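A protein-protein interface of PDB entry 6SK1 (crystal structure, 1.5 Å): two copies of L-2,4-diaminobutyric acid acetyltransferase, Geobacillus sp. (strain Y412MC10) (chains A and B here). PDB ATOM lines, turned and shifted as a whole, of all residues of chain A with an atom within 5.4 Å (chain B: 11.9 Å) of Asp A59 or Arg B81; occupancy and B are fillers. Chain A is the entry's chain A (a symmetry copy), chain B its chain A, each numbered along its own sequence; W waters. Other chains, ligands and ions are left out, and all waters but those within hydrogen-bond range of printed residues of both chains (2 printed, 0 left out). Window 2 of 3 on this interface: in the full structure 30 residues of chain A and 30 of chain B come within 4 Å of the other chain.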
ATOM      1  N   ARG A  23      -1.307  -9.290  29.582  1.00  0.00           N
ATOM      2  CA  ARG A  23      -2.505  -9.440  28.753  1.00  0.00           C
ATOM      3  C   ARG A  23      -2.238 -10.465  27.696  1.00  0.00           C
ATOM      4  O   ARG A  23      -1.156 -10.539  27.091  1.00  0.00           O
ATOM      5  CB  ARG A  23      -2.794  -8.138  28.050  1.00  0.00           C
ATOM      6  CG  ARG A  23      -3.060  -6.963  28.920  1.00  0.00           C
ATOM      7  CD  ARG A  23      -3.978  -7.211  30.017  1.00  0.00           C
ATOM      8  NE  ARG A  23      -4.456  -5.996  30.651  1.00  0.00           N
ATOM      9  CZ  ARG A  23      -5.391  -5.913  31.573  1.00  0.00           C
ATOM     10  NH1 ARG A  23      -5.778  -4.729  32.080  1.00  0.00           N
ATOM     11  NH2 ARG A  23      -6.035  -7.015  31.949  1.00  0.00           N
ATOM     12  N   ASP A  55      -7.458  -9.843  20.878  1.00  0.00           N
ATOM     13  CA  ASP A  55      -7.502  -8.584  20.171  1.00  0.00           C
ATOM     14  C   ASP A  55      -8.561  -7.649  20.668  1.00  0.00           C
ATOM     15  O   ASP A  55      -8.441  -6.397  20.509  1.00  0.00           O
ATOM     16  CB  ASP A  55      -7.769  -8.759  18.650  1.00  0.00           C
ATOM     17  CG  ASP A  55      -6.530  -8.806  17.813  1.00  0.00           C
ATOM     18  OD1 ASP A  55      -5.481  -8.289  18.213  1.00  0.00           O
ATOM     19  OD2 ASP A  55      -6.628  -9.396  16.717  1.00  0.00           O
ATOM     20  N   TYR A  56      -9.655  -8.138  21.218  1.00  0.00           N
ATOM     21  CA  TYR A  56     -10.811  -7.271  21.543  1.00  0.00           C
ATOM     22  C   TYR A  56     -11.214  -7.231  23.008  1.00  0.00           C
ATOM     23  O   TYR A  56     -11.903  -6.284  23.389  1.00  0.00           O
ATOM     24  CB  TYR A  56     -12.034  -7.722  20.689  1.00  0.00           C
ATOM     25  CG  TYR A  56     -11.804  -7.513  19.229  1.00  0.00           C
ATOM     26  CD1 TYR A  56     -11.926  -6.262  18.667  1.00  0.00           C
ATOM     27  CD2 TYR A  56     -11.496  -8.547  18.385  1.00  0.00           C
ATOM     28  CE1 TYR A  56     -11.659  -6.046  17.310  1.00  0.00           C
ATOM     29  CE2 TYR A  56     -11.193  -8.351  17.055  1.00  0.00           C
ATOM     30  CZ  TYR A  56     -11.274  -7.060  16.578  1.00  0.00           C
ATOM     31  OH  TYR A  56     -10.993  -6.853  15.218  1.00  0.00           O
ATOM     32  N   PHE A  57     -10.840  -8.224  23.802  1.00  0.00           N
ATOM     33  CA  PHE A  57     -11.217  -8.262  25.185  1.00  0.00           C
ATOM     34  C   PHE A  57     -10.018  -8.251  26.111  1.00  0.00           C
ATOM     35  O   PHE A  57     -10.194  -8.631  27.334  1.00  0.00           O
ATOM     36  CB  PHE A  57     -12.118  -9.499  25.459  1.00  0.00           C
ATOM     37  CG  PHE A  57     -13.505  -9.353  24.882  1.00  0.00           C
ATOM     38  CD1 PHE A  57     -13.753  -9.640  23.556  1.00  0.00           C
ATOM     39  CD2 PHE A  57     -14.540  -8.812  25.626  1.00  0.00           C
ATOM     40  CE1 PHE A  57     -14.992  -9.449  23.007  1.00  0.00           C
ATOM     41  CE2 PHE A  57     -15.816  -8.650  25.056  1.00  0.00           C
ATOM     42  CZ  PHE A  57     -16.029  -8.921  23.762  1.00  0.00           C
ATOM     43  N   ASN A  58      -8.865  -7.818  25.646  1.00  0.00           N
ATOM     44  CA  ASN A  58      -7.704  -8.179  26.490  1.00  0.00           C
ATOM     45  C   ASN A  58      -7.610  -7.233  27.677  1.00  0.00           C
ATOM     46  O   ASN A  58      -6.954  -7.626  28.642  1.00  0.00           O
ATOM     47  CB  ASN A  58      -6.449  -8.434  25.666  1.00  0.00           C
ATOM     48  CG  ASN A  58      -5.876  -7.184  25.207  1.00  0.00           C
ATOM     49  OD1 ASN A  58      -6.510  -6.151  25.221  1.00  0.00           O
ATOM     50  ND2 ASN A  58      -4.719  -7.360  24.582  1.00  0.00           N
ATOM     51  N   ASP A  59      -8.394  -6.165  27.780  1.00  0.00           N
ATOM     52  CA  ASP A  59      -8.378  -5.333  28.942  1.00  0.00           C
ATOM     53  C   ASP A  59      -9.031  -6.004  30.148  1.00  0.00           C
ATOM     54  O   ASP A  59      -8.864  -5.571  31.285  1.00  0.00           O
ATOM     55  CB  ASP A  59      -9.112  -3.958  28.723  1.00  0.00           C
ATOM     56  CG  ASP A  59      -8.414  -3.055  27.768  1.00  0.00           C
ATOM     57  OD1 ASP A  59      -7.217  -2.948  27.797  1.00  0.00           O
ATOM     58  OD2 ASP A  59      -9.167  -2.592  26.839  1.00  0.00           O
ATOM     59  N   THR A  60      -9.788  -7.083  29.882  1.00  0.00           N
ATOM     60  CA  THR A  60     -10.471  -7.856  30.886  1.00  0.00           C
ATOM     61  C   THR A  60     -10.037  -9.300  30.885  1.00  0.00           C
ATOM     62  O   THR A  60     -10.791 -10.165  31.411  1.00  0.00           O
ATOM     63  CB  THR A  60     -11.991  -7.742  30.816  1.00  0.00           C
ATOM     64  OG1 THR A  60     -12.433  -8.010  29.507  1.00  0.00           O
ATOM     65  CG2 THR A  60     -12.368  -6.296  31.143  1.00  0.00           C
ATOM     66  N   CYS A  61      -8.828  -9.597  30.398  1.00  0.00           N
ATOM     67  CA  CYS A  61      -8.237 -10.924  30.461  1.00  0.00           C
ATOM     68  C   CYS A  61      -6.842 -10.836  31.011  1.00  0.00           C
ATOM     69  O   CYS A  61      -6.200  -9.767  31.019  1.00  0.00           O
ATOM     70  CB  CYS A  61      -8.194 -11.596  29.075  1.00  0.00           C
ATOM     71  SG  CYS A  61      -9.835 -11.833  28.306  1.00  0.00           S
ATOM     72  N   LEU A 110      -6.210  -8.663  37.715  1.00  0.00           N
ATOM     73  CA  LEU A 110      -7.195  -8.186  36.780  1.00  0.00           C
ATOM     74  C   LEU A 110      -8.001  -7.051  37.372  1.00  0.00           C
ATOM     75  O   LEU A 110      -8.285  -5.983  36.752  1.00  0.00           O
ATOM     76  CB  LEU A 110      -8.047  -9.400  36.451  1.00  0.00           C
ATOM     77  CG  LEU A 110      -8.959  -9.301  35.337  1.00  0.00           C
ATOM     78  CD1 LEU A 110      -8.213  -9.270  34.003  1.00  0.00           C
ATOM     79  CD2 LEU A 110     -10.029 -10.467  35.310  1.00  0.00           C
ATOM     80  N   ALA A 115      -8.557  -0.743  33.719  1.00  0.00           N
ATOM     81  CA  ALA A 115      -9.650  -1.325  32.925  1.00  0.00           C
ATOM     82  C   ALA A 115     -10.793  -1.850  33.721  1.00  0.00           C
ATOM     83  O   ALA A 115     -11.926  -1.954  33.190  1.00  0.00           O
ATOM     84  CB  ALA A 115      -9.067  -2.471  32.078  1.00  0.00           C
ATOM     85  N   CYS A 116     -10.573  -2.166  35.005  1.00  0.00           N
ATOM     86  CA  CYS A 116     -11.628  -2.612  35.898  1.00  0.00           C
ATOM     87  C   CYS A 116     -12.079  -1.634  36.917  1.00  0.00           C
ATOM     88  O   CYS A 116     -12.797  -1.966  37.851  1.00  0.00           O
ATOM     89  CB  CYS A 116     -11.268  -3.965  36.549  1.00  0.00           C
ATOM     90  SG  CYS A 116     -11.275  -5.344  35.368  1.00  0.00           S
ATOM     91  N   PHE B  57     -25.035 -11.078  25.603  1.00  0.00           N
ATOM     92  CA  PHE B  57     -24.764 -10.431  24.353  1.00  0.00           C
ATOM     93  C   PHE B  57     -25.964 -10.435  23.428  1.00  0.00           C
ATOM     94  O   PHE B  57     -25.761 -10.211  22.171  1.00  0.00           O
ATOM     95  CB  PHE B  57     -23.534 -11.090  23.667  1.00  0.00           C
ATOM     96  CG  PHE B  57     -22.232 -10.751  24.350  1.00  0.00           C
ATOM     97  CD1 PHE B  57     -21.812 -11.452  25.461  1.00  0.00           C
ATOM     98  CD2 PHE B  57     -21.480  -9.655  23.961  1.00  0.00           C
ATOM     99  CE1 PHE B  57     -20.665 -11.111  26.126  1.00  0.00           C
ATOM    100  CE2 PHE B  57     -20.288  -9.334  24.635  1.00  0.00           C
ATOM    101  CZ  PHE B  57     -19.909 -10.019  25.722  1.00  0.00           C
ATOM    102  N   PHE B  77     -20.397  -8.637  18.747  1.00  0.00           N
ATOM    103  CA  PHE B  77     -20.204  -7.791  19.940  1.00  0.00           C
ATOM    104  C   PHE B  77     -19.793  -6.407  19.481  1.00  0.00           C
ATOM    105  O   PHE B  77     -19.133  -6.225  18.450  1.00  0.00           O
ATOM    106  CB  PHE B  77     -19.127  -8.392  20.897  1.00  0.00           C
ATOM    107  CG  PHE B  77     -17.810  -8.662  20.300  1.00  0.00           C
ATOM    108  CD1 PHE B  77     -16.848  -7.651  20.211  1.00  0.00           C
ATOM    109  CD2 PHE B  77     -17.494  -9.889  19.757  1.00  0.00           C
ATOM    110  CE1 PHE B  77     -15.600  -7.919  19.659  1.00  0.00           C
ATOM    111  CE2 PHE B  77     -16.238 -10.134  19.237  1.00  0.00           C
ATOM    112  CZ  PHE B  77     -15.309  -9.116  19.159  1.00  0.00           C
ATOM    113  N   ARG B  78     -20.145  -5.433  20.303  1.00  0.00           N
ATOM    114  CA  ARG B  78     -19.561  -4.098  20.119  1.00  0.00           C
ATOM    115  C   ARG B  78     -18.179  -4.109  20.769  1.00  0.00           C
ATOM    116  O   ARG B  78     -18.032  -4.562  21.919  1.00  0.00           O
ATOM    117  CB  ARG B  78     -20.471  -3.036  20.718  1.00  0.00           C
ATOM    118  CG  ARG B  78     -21.770  -2.922  19.885  1.00  0.00           C
ATOM    119  CD  ARG B  78     -22.902  -1.916  20.178  1.00  0.00           C
ATOM    120  NE  ARG B  78     -22.409  -0.629  19.725  1.00  0.00           N
ATOM    121  CZ  ARG B  78     -23.181   0.382  19.451  1.00  0.00           C
ATOM    122  NH1 ARG B  78     -22.568   1.475  19.145  1.00  0.00           N
ATOM    123  NH2 ARG B  78     -24.559   0.333  19.439  1.00  0.00           N
ATOM    124  N   SER B  79     -17.150  -3.700  20.055  1.00  0.00           N
ATOM    125  CA  SER B  79     -15.827  -3.772  20.571  1.00  0.00           C
ATOM    126  C   SER B  79     -15.687  -2.983  21.842  1.00  0.00           C
ATOM    127  O   SER B  79     -16.010  -1.797  21.879  1.00  0.00           O
ATOM    128  CB  SER B  79     -14.873  -3.204  19.528  1.00  0.00           C
ATOM    129  OG  SER B  79     -13.553  -3.111  20.063  1.00  0.00           O
ATOM    130  N   PRO B  80     -15.186  -3.567  22.938  1.00  0.00           N
ATOM    131  CA  PRO B  80     -15.070  -2.802  24.199  1.00  0.00           C
ATOM    132  C   PRO B  80     -14.307  -1.486  24.012  1.00  0.00           C
ATOM    133  O   PRO B  80     -14.744  -0.437  24.576  1.00  0.00           O
ATOM    134  CB  PRO B  80     -14.391  -3.806  25.156  1.00  0.00           C
ATOM    135  CG  PRO B  80     -14.895  -5.114  24.678  1.00  0.00           C
ATOM    136  CD  PRO B  80     -14.995  -5.021  23.139  1.00  0.00           C
ATOM    137  N   ARG B  81     -13.180  -1.505  23.351  1.00  0.00           N
ATOM    138  CA  ARG B  81     -12.379  -0.294  23.229  1.00  0.00           C
ATOM    139  C   ARG B  81     -13.027   0.698  22.264  1.00  0.00           C
ATOM    140  O   ARG B  81     -12.694   1.898  22.314  1.00  0.00           O
ATOM    141  CB  ARG B  81     -11.021  -0.570  22.763  1.00  0.00           C
ATOM    142  CG  ARG B  81     -10.157  -1.208  23.850  1.00  0.00           C
ATOM    143  CD  ARG B  81      -8.801  -1.502  23.312  1.00  0.00           C
ATOM    144  NE  ARG B  81      -7.930  -2.087  24.319  1.00  0.00           N
ATOM    145  CZ  ARG B  81      -6.746  -2.639  24.052  1.00  0.00           C
ATOM    146  NH1 ARG B  81      -6.066  -3.124  25.085  1.00  0.00           N
ATOM    147  NH2 ARG B  81      -6.272  -2.721  22.855  1.00  0.00           N
ATOM    148  N   ASN B  82     -13.767   0.222  21.279  1.00  0.00           N
ATOM    149  CA  ASN B  82     -14.258   1.056  20.168  1.00  0.00           C
ATOM    150  C   ASN B  82     -15.724   0.658  19.874  1.00  0.00           C
ATOM    151  O   ASN B  82     -15.931  -0.127  18.935  1.00  0.00           O
ATOM    152  CB  ASN B  82     -13.411   0.891  19.015  1.00  0.00           C
ATOM    153  CG  ASN B  82     -12.031   1.460  19.240  1.00  0.00           C
ATOM    154  OD1 ASN B  82     -11.874   2.648  19.432  1.00  0.00           O
ATOM    155  ND2 ASN B  82     -11.065   0.611  19.167  1.00  0.00           N
ATOM    156  N   PRO B  83     -16.641   1.113  20.709  1.00  0.00           N
ATOM    157  CA  PRO B  83     -18.013   0.586  20.568  1.00  0.00           C
ATOM    158  C   PRO B  83     -18.736   0.968  19.293  1.00  0.00           C
ATOM    159  O   PRO B  83     -19.808   0.369  19.093  1.00  0.00           O
ATOM    160  CB  PRO B  83     -18.674   1.109  21.789  1.00  0.00           C
ATOM    161  CG  PRO B  83     -17.804   2.127  22.420  1.00  0.00           C
ATOM    162  CD  PRO B  83     -16.462   1.971  21.916  1.00  0.00           C
ATOM    163  N   GLU B  84     -18.214   1.815  18.481  1.00  0.00           N
ATOM    164  CA  GLU B  84     -18.793   2.033  17.181  1.00  0.00           C
ATOM    165  C   GLU B  84     -18.454   0.918  16.174  1.00  0.00           C
ATOM    166  O   GLU B  84     -18.940   0.898  15.048  1.00  0.00           O
ATOM    167  CB  GLU B  84     -18.357   3.388  16.611  1.00  0.00           C
ATOM    168  CG  GLU B  84     -19.059   4.503  17.455  1.00  0.00           C
ATOM    169  CD  GLU B  84     -18.798   5.929  16.937  1.00  0.00           C
ATOM    170  OE1 GLU B  84     -19.403   6.838  17.510  1.00  0.00           O
ATOM    171  OE2 GLU B  84     -18.050   6.162  15.987  1.00  0.00           O
ATOM    172  N   THR B  85     -17.614  -0.036  16.557  1.00  0.00           N
ATOM    173  CA  THR B  85     -17.305  -1.202  15.778  1.00  0.00           C
ATOM    174  C   THR B  85     -18.147  -2.365  16.282  1.00  0.00           C
ATOM    175  O   THR B  85     -18.049  -2.753  17.439  1.00  0.00           O
ATOM    176  CB  THR B  85     -15.862  -1.593  15.872  1.00  0.00           C
ATOM    177  OG1 THR B  85     -15.035  -0.569  15.279  1.00  0.00           O
ATOM    178  CG2 THR B  85     -15.561  -2.874  15.147  1.00  0.00           C
ATOM    179  N   LEU B  86     -18.888  -2.955  15.358  1.00  0.00           N
ATOM    180  CA  LEU B  86     -19.626  -4.217  15.611  1.00  0.00           C
ATOM    181  C   LEU B  86     -18.795  -5.309  14.977  1.00  0.00           C
ATOM    182  O   LEU B  86     -18.658  -5.300  13.728  1.00  0.00           O
ATOM    183  CB  LEU B  86     -21.015  -4.174  14.990  1.00  0.00           C
ATOM    184  CG  LEU B  86     -21.861  -5.397  15.351  1.00  0.00           C
ATOM    185  CD1 LEU B  86     -22.264  -5.452  16.816  1.00  0.00           C
ATOM    186  CD2 LEU B  86     -23.008  -5.519  14.420  1.00  0.00           C
ATOM    187  N   PHE B  87     -18.254  -6.237  15.772  1.00  0.00           N
ATOM    188  CA  PHE B  87     -17.498  -7.343  15.228  1.00  0.00           C
ATOM    189  C   PHE B  87     -18.434  -8.530  15.138  1.00  0.00           C
ATOM    190  O   PHE B  87     -18.934  -8.995  16.193  1.00  0.00           O
ATOM    191  CB  PHE B  87     -16.271  -7.648  16.073  1.00  0.00           C
ATOM    192  CG  PHE B  87     -15.320  -8.576  15.410  1.00  0.00           C
ATOM    193  CD1 PHE B  87     -15.583  -9.910  15.395  1.00  0.00           C
ATOM    194  CD2 PHE B  87     -14.192  -8.119  14.782  1.00  0.00           C
ATOM    195  CE1 PHE B  87     -14.771 -10.757  14.729  1.00  0.00           C
ATOM    196  CE2 PHE B  87     -13.395  -8.948  14.078  1.00  0.00           C
ATOM    197  CZ  PHE B  87     -13.653 -10.280  14.036  1.00  0.00           C
ATOM    198  N   GLY B 118     -25.644   3.700  16.207  1.00  0.00           N
ATOM    199  CA  GLY B 118     -24.341   4.224  16.523  1.00  0.00           C
ATOM    200  C   GLY B 118     -23.180   3.346  15.996  1.00  0.00           C
ATOM    201  O   GLY B 118     -22.029   3.810  16.015  1.00  0.00           O
ATOM    202  N   ARG B 120     -20.755   2.275  13.425  1.00  0.00           N
ATOM    203  CA  ARG B 120     -20.253   2.877  12.220  1.00  0.00           C
ATOM    204  C   ARG B 120     -19.449   1.956  11.347  1.00  0.00           C
ATOM    205  O   ARG B 120     -19.289   2.218  10.156  1.00  0.00           O
ATOM    206  CB  ARG B 120     -19.406   4.170  12.464  1.00  0.00           C
ATOM    207  CG  ARG B 120     -20.035   5.238  13.347  1.00  0.00           C
ATOM    208  CD  ARG B 120     -19.425   6.641  13.143  1.00  0.00           C
ATOM    209  NE  ARG B 120     -17.989   6.682  12.785  1.00  0.00           N
ATOM    210  CZ  ARG B 120     -17.491   7.322  11.723  1.00  0.00           C
ATOM    211  NH1 ARG B 120     -18.321   7.926  10.886  1.00  0.00           N
ATOM    212  NH2 ARG B 120     -16.172   7.317  11.452  1.00  0.00           N
ATOM    213  N   PHE B 121     -18.940   0.860  11.918  1.00  0.00           N
ATOM    214  CA  PHE B 121     -18.194  -0.142  11.153  1.00  0.00           C
ATOM    215  C   PHE B 121     -18.693  -1.529  11.499  1.00  0.00           C
ATOM    216  O   PHE B 121     -18.827  -1.798  12.708  1.00  0.00           O
ATOM    217  CB  PHE B 121     -16.675  -0.036  11.397  1.00  0.00           C
ATOM    218  CG  PHE B 121     -16.074   1.234  10.820  1.00  0.00           C
ATOM    219  CD1 PHE B 121     -16.090   2.384  11.601  1.00  0.00           C
ATOM    220  CD2 PHE B 121     -15.519   1.246   9.602  1.00  0.00           C
ATOM    221  CE1 PHE B 121     -15.540   3.539  11.075  1.00  0.00           C
ATOM    222  CE2 PHE B 121     -14.956   2.442   9.079  1.00  0.00           C
ATOM    223  CZ  PHE B 121     -15.016   3.551   9.780  1.00  0.00           C
ATOM    224  N   GLU B 123     -17.087  -5.310  11.273  1.00  0.00           N
ATOM    225  CA  GLU B 123     -15.804  -6.015  11.058  1.00  0.00           C
ATOM    226  C   GLU B 123     -16.079  -7.517  11.261  1.00  0.00           C
ATOM    227  O   GLU B 123     -16.820  -7.909  12.143  1.00  0.00           O
ATOM    228  CB  GLU B 123     -14.726  -5.523  11.941  1.00  0.00           C
ATOM    229  CG  GLU B 123     -14.513  -4.018  11.680  1.00  0.00           C
ATOM    230  CD  GLU B 123     -13.367  -3.426  12.379  1.00  0.00           C
ATOM    231  OE1 GLU B 123     -12.616  -4.096  13.125  1.00  0.00           O
ATOM    232  OE2 GLU B 123     -13.260  -2.150  12.309  1.00  0.00           O
ATOM    233  N   TYR B 154      -6.275 -13.171  10.687  1.00  0.00           N
ATOM    234  CA  TYR B 154      -5.606 -14.262  11.416  1.00  0.00           C
ATOM    235  C   TYR B 154      -5.183 -15.292  10.378  1.00  0.00           C
ATOM    236  O   TYR B 154      -6.052 -16.025   9.847  1.00  0.00           O
ATOM    237  CB  TYR B 154      -6.545 -14.895  12.475  1.00  0.00           C
ATOM    238  CG  TYR B 154      -7.143 -13.852  13.417  1.00  0.00           C
ATOM    239  CD1 TYR B 154      -6.347 -13.160  14.290  1.00  0.00           C
ATOM    240  CD2 TYR B 154      -8.415 -13.441  13.298  1.00  0.00           C
ATOM    241  CE1 TYR B 154      -6.805 -12.180  15.085  1.00  0.00           C
ATOM    242  CE2 TYR B 154      -8.880 -12.406  14.078  1.00  0.00           C
ATOM    243  CZ  TYR B 154      -8.064 -11.835  15.027  1.00  0.00           C
ATOM    244  OH  TYR B 154      -8.602 -10.760  15.750  1.00  0.00           O
HETATM  245  O   HOH W   1      -9.529  -8.716  14.044  1.00  0.00           O
HETATM  246  O   HOH W   2     -11.911  -3.848  22.088  1.00  0.00           O
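NH1 of Arg B81 lies within hydrogen-bond range of OD1 of Asn A58 (3.1 Å).
The guanidinium group (NE) of Arg B81 is in salt-bridge range of the side-chain carboxylate (OD2) of Asp A59 (2.9 Å).
OD2 of Asp A55 is in hydrogen-bond range of OH of Tyr B154, at 2.6 Å.
The side-chain sulfur (SG) of Cys A61 sits at hydrogen-bond distance from the backbone carbonyl oxygen (O) of Phe A57 (3.4 Å).
The backbone carbonyl oxygen of Leu B86 lies within hydrogen-bond range of the backbone NH of Glu B123 (2.9 Å).
The backbone carbonyl oxygen of Asn A58 lies close to the guanidinium group of Arg A23 (3.5 Å).
The backbone carbonyl oxygen of Phe B77 sits at hydrogen-bond distance from the backbone NH of Phe B87 (2.8 Å).
The backbone NH of Ser B79 sits at hydrogen-bond distance from the backbone carbonyl oxygen of Thr B85, at 2.9 Å.
The backbone carbonyl oxygen (O) of Asp A59 is in hydrogen-bond range of the guanidinium group (NH2) of Arg A23, at 3.2 Å.
Among the printed residues, pairs that only touch across the chains: Tyr A56 with Pro B80 (3.3 Å), Tyr A56 with Phe B87 (3.4 Å), Phe A57 with Pro B80 (3.7 Å), Tyr A56 with Phe B77 (3.7 Å), Phe A57 with Phe B77 (3.7 Å), Tyr A56 with Tyr B154 (3.8 Å), Tyr A56 with Ser B79 (3.8 Å) and Tyr A56 with Glu B123 (3.8 Å).
Of chain B, only Arg B81 comes within 4 Å of Asp A59.
Arg B81 touches two residues of chain A.
Asn A58 touches one residue of chain B.
No residue of chain B comes within 4 Å of Thr A60.
No residue of chain B comes within 4 Å of Cys A61.
Leu A110 touches none of the printed residues of chain B.
No residue of chain B comes within 4 Å of Ala A115.
Of the printed residues of chain A, Phe B87 touches Tyr A56 (3.4 Å).
Of the printed residues of chain B, Asp A55 touches Tyr B154 (2.6 Å).
Of the printed residues of chain A, Phe B77 touches Tyr A56 (3.7 Å) and Phe A57 (3.7 Å).
Leu B86 touches none of the printed residues of chain A.
Pro B83 touches none of the printed residues of chain A.
The nearest residue of chain B that does not touch Asp A59 is Pro B80 (5.6 Å).
The nearest printed residue of chain A that does not touch Glu B123 is Asp A55 (8.7 Å).
Of the 17 printed residues of chain B, 7 touch a printed residue of chain A.
Of the 11 printed residues of chain A, 5 touch a printed residue of chain B.
Among the printed residues, 11 pairs touch across the chains.
Among the printed residues, Asp or Glu carboxylates within 4 Å of a Lys or Arg side-chain nitrogen of the other chain: Asp A59 with Arg B81 (2.9 Å).
Position printed for both chains: 57.
Water W1 lies within hydrogen-bond range of OH of Tyr A56 (2.6 Å) and OH of Tyr B154 (2.8 Å).
Water W2 lies within hydrogen-bond range of the side-chain hydroxyl of Ser B79 (2.7 Å), the backbone carbonyl oxygen of Tyr A56 (2.8 Å) and the backbone NH of Arg B81 (2.9 Å).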
